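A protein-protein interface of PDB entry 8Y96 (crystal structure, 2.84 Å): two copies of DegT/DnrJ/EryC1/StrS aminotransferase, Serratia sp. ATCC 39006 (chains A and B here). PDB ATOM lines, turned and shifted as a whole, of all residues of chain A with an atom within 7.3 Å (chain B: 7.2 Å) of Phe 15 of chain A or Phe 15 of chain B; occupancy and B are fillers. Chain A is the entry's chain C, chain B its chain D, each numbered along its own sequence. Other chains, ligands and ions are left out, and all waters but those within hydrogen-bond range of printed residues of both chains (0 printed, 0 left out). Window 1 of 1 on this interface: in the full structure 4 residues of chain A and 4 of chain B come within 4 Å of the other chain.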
ATOM      1  N   GLU A  12      27.837   3.372  15.651  1.00  0.00           N
ATOM      2  CA  GLU A  12      27.409   1.946  15.661  1.00  0.00           C
ATOM      3  C   GLU A  12      26.388   1.714  16.775  1.00  0.00           C
ATOM      4  O   GLU A  12      25.330   1.141  16.525  1.00  0.00           O
ATOM      5  CB  GLU A  12      28.605   1.001  15.803  1.00  0.00           C
ATOM      6  N   GLN A  13      26.708   2.159  18.001  1.00  0.00           N
ATOM      7  CA  GLN A  13      25.838   1.934  19.147  1.00  0.00           C
ATOM      8  C   GLN A  13      24.549   2.744  18.994  1.00  0.00           C
ATOM      9  O   GLN A  13      23.466   2.248  19.303  1.00  0.00           O
ATOM     10  CB  GLN A  13      26.502   2.283  20.478  1.00  0.00           C
ATOM     11  CG  GLN A  13      25.797   1.667  21.682  1.00  0.00           C
ATOM     12  CD  GLN A  13      25.854   2.533  22.922  1.00  0.00           C
ATOM     13  OE1 GLN A  13      24.839   3.083  23.368  1.00  0.00           O
ATOM     14  NE2 GLN A  13      27.044   2.679  23.485  1.00  0.00           N
ATOM     15  N   LEU A  14      24.676   3.990  18.519  1.00  0.00           N
ATOM     16  CA  LEU A  14      23.527   4.849  18.274  1.00  0.00           C
ATOM     17  C   LEU A  14      22.572   4.190  17.279  1.00  0.00           C
ATOM     18  O   LEU A  14      21.363   4.385  17.376  1.00  0.00           O
ATOM     19  CB  LEU A  14      23.982   6.218  17.769  1.00  0.00           C
ATOM     20  CG  LEU A  14      24.748   7.089  18.769  1.00  0.00           C
ATOM     21  CD1 LEU A  14      25.302   8.325  18.086  1.00  0.00           C
ATOM     22  CD2 LEU A  14      23.874   7.482  19.946  1.00  0.00           C
ATOM     23  N   PHE A  15      23.119   3.421  16.326  1.00  0.00           N
ATOM     24  CA  PHE A  15      22.317   2.737  15.325  1.00  0.00           C
ATOM     25  C   PHE A  15      21.585   1.552  15.954  1.00  0.00           C
ATOM     26  O   PHE A  15      20.396   1.359  15.718  1.00  0.00           O
ATOM     27  CB  PHE A  15      23.165   2.263  14.141  1.00  0.00           C
ATOM     28  CG  PHE A  15      22.372   1.431  13.144  1.00  0.00           C
ATOM     29  CD1 PHE A  15      21.464   2.034  12.280  1.00  0.00           C
ATOM     30  CD2 PHE A  15      22.518   0.050  13.083  1.00  0.00           C
ATOM     31  CE1 PHE A  15      20.729   1.280  11.380  1.00  0.00           C
ATOM     32  CE2 PHE A  15      21.784  -0.699  12.177  1.00  0.00           C
ATOM     33  CZ  PHE A  15      20.892  -0.085  11.329  1.00  0.00           C
ATOM     34  N   GLN A  16      22.313   0.754  16.741  1.00  0.00           N
ATOM     35  CA  GLN A  16      21.763  -0.452  17.340  1.00  0.00           C
ATOM     36  C   GLN A  16      20.622  -0.095  18.291  1.00  0.00           C
ATOM     37  O   GLN A  16      19.659  -0.849  18.389  1.00  0.00           O
ATOM     38  CB  GLN A  16      22.888  -1.252  17.997  1.00  0.00           C
ATOM     39  CG  GLN A  16      23.761  -1.999  16.991  1.00  0.00           C
ATOM     40  CD  GLN A  16      25.208  -2.135  17.421  1.00  0.00           C
ATOM     41  OE1 GLN A  16      25.520  -2.712  18.469  1.00  0.00           O
ATOM     42  NE2 GLN A  16      26.113  -1.606  16.610  1.00  0.00           N
ATOM     43  N   VAL A  17      20.734   1.057  18.968  1.00  0.00           N
ATOM     44  CA  VAL A  17      19.697   1.541  19.867  1.00  0.00           C
ATOM     45  C   VAL A  17      18.486   1.975  19.046  1.00  0.00           C
ATOM     46  O   VAL A  17      17.368   1.534  19.304  1.00  0.00           O
ATOM     47  CB  VAL A  17      20.193   2.697  20.759  1.00  0.00           C
ATOM     48  CG1 VAL A  17      19.060   3.353  21.541  1.00  0.00           C
ATOM     49  CG2 VAL A  17      21.293   2.240  21.708  1.00  0.00           C
ATOM     50  N   SER A  18      18.725   2.853  18.069  1.00  0.00           N
ATOM     51  CA  SER A  18      17.666   3.371  17.217  1.00  0.00           C
ATOM     52  C   SER A  18      16.876   2.227  16.587  1.00  0.00           C
ATOM     53  O   SER A  18      15.654   2.292  16.491  1.00  0.00           O
ATOM     54  CB  SER A  18      18.220   4.295  16.154  1.00  0.00           C
ATOM     55  OG  SER A  18      18.748   5.486  16.721  1.00  0.00           O
ATOM     56  N   PHE A  19      17.591   1.187  16.148  1.00  0.00           N
ATOM     57  CA  PHE A  19      16.976   0.093  15.415  1.00  0.00           C
ATOM     58  C   PHE A  19      15.971  -0.623  16.316  1.00  0.00           C
ATOM     59  O   PHE A  19      14.832  -0.865  15.917  1.00  0.00           O
ATOM     60  CB  PHE A  19      18.059  -0.853  14.884  1.00  0.00           C
ATOM     61  CG  PHE A  19      17.518  -1.991  14.031  1.00  0.00           C
ATOM     62  CD1 PHE A  19      17.002  -3.140  14.622  1.00  0.00           C
ATOM     63  CD2 PHE A  19      17.516  -1.902  12.643  1.00  0.00           C
ATOM     64  CE1 PHE A  19      16.494  -4.167  13.844  1.00  0.00           C
ATOM     65  CE2 PHE A  19      17.010  -2.936  11.869  1.00  0.00           C
ATOM     66  CZ  PHE A  19      16.501  -4.067  12.470  1.00  0.00           C
ATOM     67  N   VAL A  20      16.416  -0.960  17.531  1.00  0.00           N
ATOM     68  CA  VAL A  20      15.583  -1.648  18.503  1.00  0.00           C
ATOM     69  C   VAL A  20      14.326  -0.826  18.796  1.00  0.00           C
ATOM     70  O   VAL A  20      13.216  -1.364  18.770  1.00  0.00           O
ATOM     71  CB  VAL A  20      16.407  -1.944  19.770  1.00  0.00           C
ATOM     72  CG1 VAL A  20      15.543  -2.115  21.013  1.00  0.00           C
ATOM     73  CG2 VAL A  20      17.287  -3.167  19.567  1.00  0.00           C
ATOM     74  N   LEU A  21      14.509   0.472  19.078  1.00  0.00           N
ATOM     75  CA  LEU A  21      13.396   1.353  19.391  1.00  0.00           C
ATOM     76  C   LEU A  21      12.451   1.422  18.196  1.00  0.00           C
ATOM     77  O   LEU A  21      11.239   1.337  18.361  1.00  0.00           O
ATOM     78  CB  LEU A  21      13.899   2.739  19.789  1.00  0.00           C
ATOM     79  CG  LEU A  21      14.673   2.818  21.108  1.00  0.00           C
ATOM     80  CD1 LEU A  21      15.232   4.214  21.290  1.00  0.00           C
ATOM     81  CD2 LEU A  21      13.827   2.435  22.315  1.00  0.00           C
ATOM     82  N   MET A 203      19.034  -5.993  23.844  1.00  0.00           N
ATOM     83  CA  MET A 203      19.917  -5.814  22.703  1.00  0.00           C
ATOM     84  C   MET A 203      21.367  -5.726  23.179  1.00  0.00           C
ATOM     85  O   MET A 203      22.215  -6.483  22.714  1.00  0.00           O
ATOM     86  CB  MET A 203      19.522  -4.565  21.906  1.00  0.00           C
ATOM     87  CG  MET A 203      20.442  -4.217  20.741  1.00  0.00           C
ATOM     88  SD  MET A 203      21.824  -3.131  21.149  1.00  0.00           S
ATOM     89  CE  MET A 203      21.046  -1.661  21.834  1.00  0.00           C
ATOM     90  N   GLU B  12      29.218   5.124   5.921  1.00  0.00           N
ATOM     91  CA  GLU B  12      30.123   4.362   6.827  1.00  0.00           C
ATOM     92  C   GLU B  12      29.475   4.190   8.201  1.00  0.00           C
ATOM     93  O   GLU B  12      29.642   3.146   8.834  1.00  0.00           O
ATOM     94  CB  GLU B  12      31.488   5.044   6.934  1.00  0.00           C
ATOM     95  N   GLN B  13      28.766   5.231   8.663  1.00  0.00           N
ATOM     96  CA  GLN B  13      27.971   5.166   9.879  1.00  0.00           C
ATOM     97  C   GLN B  13      26.501   4.952   9.522  1.00  0.00           C
ATOM     98  O   GLN B  13      25.912   5.747   8.794  1.00  0.00           O
ATOM     99  CB  GLN B  13      28.138   6.423  10.733  1.00  0.00           C
ATOM    100  CG  GLN B  13      29.137   6.276  11.877  1.00  0.00           C
ATOM    101  CD  GLN B  13      28.483   5.900  13.191  1.00  0.00           C
ATOM    102  OE1 GLN B  13      27.749   4.908  13.294  1.00  0.00           O
ATOM    103  NE2 GLN B  13      28.733   6.708  14.212  1.00  0.00           N
ATOM    104  N   LEU B  14      25.926   3.876  10.072  1.00  0.00           N
ATOM    105  CA  LEU B  14      24.559   3.476   9.787  1.00  0.00           C
ATOM    106  C   LEU B  14      23.590   4.485  10.399  1.00  0.00           C
ATOM    107  O   LEU B  14      22.511   4.724   9.863  1.00  0.00           O
ATOM    108  CB  LEU B  14      24.333   2.069  10.340  1.00  0.00           C
ATOM    109  CG  LEU B  14      25.171   0.945   9.718  1.00  0.00           C
ATOM    110  CD1 LEU B  14      25.105  -0.300  10.588  1.00  0.00           C
ATOM    111  CD2 LEU B  14      24.736   0.613   8.297  1.00  0.00           C
ATOM    112  N   PHE B  15      23.993   5.082  11.523  1.00  0.00           N
ATOM    113  CA  PHE B  15      23.151   6.033  12.223  1.00  0.00           C
ATOM    114  C   PHE B  15      23.014   7.317  11.410  1.00  0.00           C
ATOM    115  O   PHE B  15      21.909   7.830  11.263  1.00  0.00           O
ATOM    116  CB  PHE B  15      23.711   6.322  13.617  1.00  0.00           C
ATOM    117  CG  PHE B  15      22.861   7.337  14.361  1.00  0.00           C
ATOM    118  CD1 PHE B  15      21.603   6.989  14.839  1.00  0.00           C
ATOM    119  CD2 PHE B  15      23.310   8.639  14.555  1.00  0.00           C
ATOM    120  CE1 PHE B  15      20.819   7.917  15.501  1.00  0.00           C
ATOM    121  CE2 PHE B  15      22.523   9.564  15.224  1.00  0.00           C
ATOM    122  CZ  PHE B  15      21.280   9.202  15.694  1.00  0.00           C
ATOM    123  N   GLN B  16      24.139   7.839  10.901  1.00  0.00           N
ATOM    124  CA  GLN B  16      24.135   9.055  10.100  1.00  0.00           C
ATOM    125  C   GLN B  16      23.181   8.924   8.912  1.00  0.00           C
ATOM    126  O   GLN B  16      22.390   9.830   8.659  1.00  0.00           O
ATOM    127  CB  GLN B  16      25.518   9.424   9.558  1.00  0.00           C
ATOM    128  CG  GLN B  16      26.309  10.386  10.440  1.00  0.00           C
ATOM    129  CD  GLN B  16      27.243   9.691  11.406  1.00  0.00           C
ATOM    130  OE1 GLN B  16      26.829   8.838  12.199  1.00  0.00           O
ATOM    131  NE2 GLN B  16      28.518  10.049  11.346  1.00  0.00           N
ATOM    132  N   VAL B  17      23.279   7.800   8.189  1.00  0.00           N
ATOM    133  CA  VAL B  17      22.486   7.559   6.993  1.00  0.00           C
ATOM    134  C   VAL B  17      21.016   7.414   7.377  1.00  0.00           C
ATOM    135  O   VAL B  17      20.146   8.002   6.738  1.00  0.00           O
ATOM    136  CB  VAL B  17      22.982   6.315   6.228  1.00  0.00           C
ATOM    137  CG1 VAL B  17      22.075   5.951   5.054  1.00  0.00           C
ATOM    138  CG2 VAL B  17      24.417   6.492   5.747  1.00  0.00           C
ATOM    139  N   SER B  18      20.753   6.607   8.410  1.00  0.00           N
ATOM    140  CA  SER B  18      19.404   6.400   8.912  1.00  0.00           C
ATOM    141  C   SER B  18      18.777   7.723   9.349  1.00  0.00           C
ATOM    142  O   SER B  18      17.609   7.979   9.068  1.00  0.00           O
ATOM    143  CB  SER B  18      19.404   5.395  10.041  1.00  0.00           C
ATOM    144  OG  SER B  18      19.810   4.116   9.571  1.00  0.00           O
ATOM    145  N   PHE B  19      19.567   8.556  10.034  1.00  0.00           N
ATOM    146  CA  PHE B  19      19.078   9.794  10.619  1.00  0.00           C
ATOM    147  C   PHE B  19      18.592  10.738   9.521  1.00  0.00           C
ATOM    148  O   PHE B  19      17.569  11.399   9.680  1.00  0.00           O
ATOM    149  CB  PHE B  19      20.167  10.456  11.472  1.00  0.00           C
ATOM    150  CG  PHE B  19      19.681  11.724  12.156  1.00  0.00           C
ATOM    151  CD1 PHE B  19      19.716  12.949  11.494  1.00  0.00           C
ATOM    152  CD2 PHE B  19      19.154  11.679  13.442  1.00  0.00           C
ATOM    153  CE1 PHE B  19      19.243  14.099  12.108  1.00  0.00           C
ATOM    154  CE2 PHE B  19      18.680  12.831  14.055  1.00  0.00           C
ATOM    155  CZ  PHE B  19      18.727  14.039  13.388  1.00  0.00           C
ATOM    156  N   VAL B  20      19.342  10.805   8.419  1.00  0.00           N
ATOM    157  CA  VAL B  20      19.034  11.733   7.342  1.00  0.00           C
ATOM    158  C   VAL B  20      17.803  11.228   6.594  1.00  0.00           C
ATOM    159  O   VAL B  20      16.894  12.001   6.306  1.00  0.00           O
ATOM    160  CB  VAL B  20      20.254  11.957   6.422  1.00  0.00           C
ATOM    161  CG1 VAL B  20      19.873  12.323   4.991  1.00  0.00           C
ATOM    162  CG2 VAL B  20      21.190  13.013   7.003  1.00  0.00           C
ATOM    163  N   LEU B  21      17.771   9.923   6.312  1.00  0.00           N
ATOM    164  CA  LEU B  21      16.636   9.316   5.641  1.00  0.00           C
ATOM    165  C   LEU B  21      15.387   9.485   6.502  1.00  0.00           C
ATOM    166  O   LEU B  21      14.313   9.802   5.990  1.00  0.00           O
ATOM    167  CB  LEU B  21      16.946   7.853   5.339  1.00  0.00           C
ATOM    168  CG  LEU B  21      18.038   7.617   4.290  1.00  0.00           C
ATOM    169  CD1 LEU B  21      18.487   6.169   4.288  1.00  0.00           C
ATOM    170  CD2 LEU B  21      17.568   8.024   2.903  1.00  0.00           C
ATOM    171  N   MET B 203      25.027  14.762   3.317  1.00  0.00           N
ATOM    172  CA  MET B 203      25.468  14.458   4.669  1.00  0.00           C
ATOM    173  C   MET B 203      26.937  14.047   4.644  1.00  0.00           C
ATOM    174  O   MET B 203      27.732  14.559   5.427  1.00  0.00           O
ATOM    175  CB  MET B 203      24.617  13.338   5.286  1.00  0.00           C
ATOM    176  CG  MET B 203      25.071  12.853   6.667  1.00  0.00           C
ATOM    177  SD  MET B 203      26.393  11.619   6.673  1.00  0.00           S
ATOM    178  CE  MET B 203      25.692  10.239   5.757  1.00  0.00           C
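The side-chain amide oxygen (OE1) of Gln 13 of chain B is in hydrogen-bond range of the backbone NH (N) of Glu 12 of chain A.
The backbone carbonyl oxygen of Glu 12 of chain A sits at hydrogen-bond distance from the side-chain amide nitrogen of Gln 16 of chain A.
OG of Ser 18 of chain A lies within hydrogen-bond range of O of Leu 14 of chain A (2.9 Å).
NE2 of Gln 13 of chain B sits close to OE1 of Gln 16 of chain B, at 3.5 Å.
O of Leu 14 of chain B lies within hydrogen-bond range of OG of Ser 18 of chain B, 2.8 Å away.
CD1 of Phe 15 of chain B touches O of Leu 14 of chain A, 3.6 Å away.
Phe 15 of chain A touches Leu 14 of chain B.
Phe 15 of chain A touches Phe 15 of chain B.
Ser 18 of chain B touches Phe 15 of chain A (OG to CE1, 3.5 Å).
Ser 18 of chain A touches Phe 15 of chain B.
Printed residues of chain B within 4 Å of Glu 12 of chain A: Gln 13.
Printed residues of chain B within 4 Å of Ser 18 of chain A: Phe 15 (3.4 Å).
Met 203 of chain A touches none of the printed residues of chain B.
Of the printed residues of chain A, Gln 13 of chain B touches Glu 12 (2.8 Å).
Of the printed residues of chain A, Leu 14 of chain B touches Phe 15.
Phe 15 of chain B touches just these residues of chain A: Leu 14 (3.6 Å), Phe 15 (3.9 Å) and Ser 18 (3.4 Å).
Leu 21 of chain B touches none of the printed residues of chain A.
The nearest residue of chain B that does not touch Phe 15 of chain A is Gln 13 of chain B (5.4 Å).
The nearest residue of chain A that does not touch Phe 15 of chain B is Glu 12 of chain A (5.5 Å).
Hydrophobic or aromatic side chains of chain B within 4 Å of the printed part of chain A: Leu 14 and Phe 15.
Among the printed residues, 6 pairs touch across the chains.
Among the printed residues, no Asp or Glu carboxylate lies within 4 Å of a Lys or Arg side-chain nitrogen of the other chain.
Glu 12 of chain A touches Gln 13 of chain B, but with the chains exchanged Gln 13 of chain A does not touch Glu 12 of chain B (9.7 Å).
Leu 14 of chain A touches Phe 15 of chain B, and with the chains exchanged Phe 15 of chain A touches Leu 14 of chain B.
Phe 15 of chain B touches its own counterpart, Phe 15 of chain A.
Phe 15 of chain A touches Ser 18 of chain B, and with the chains exchanged Ser 18 of chain A touches Phe 15 of chain B.
Of the 6 pairs that touch across the chains among the printed residues, 5 have their exchanged pair printed and touching as well.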
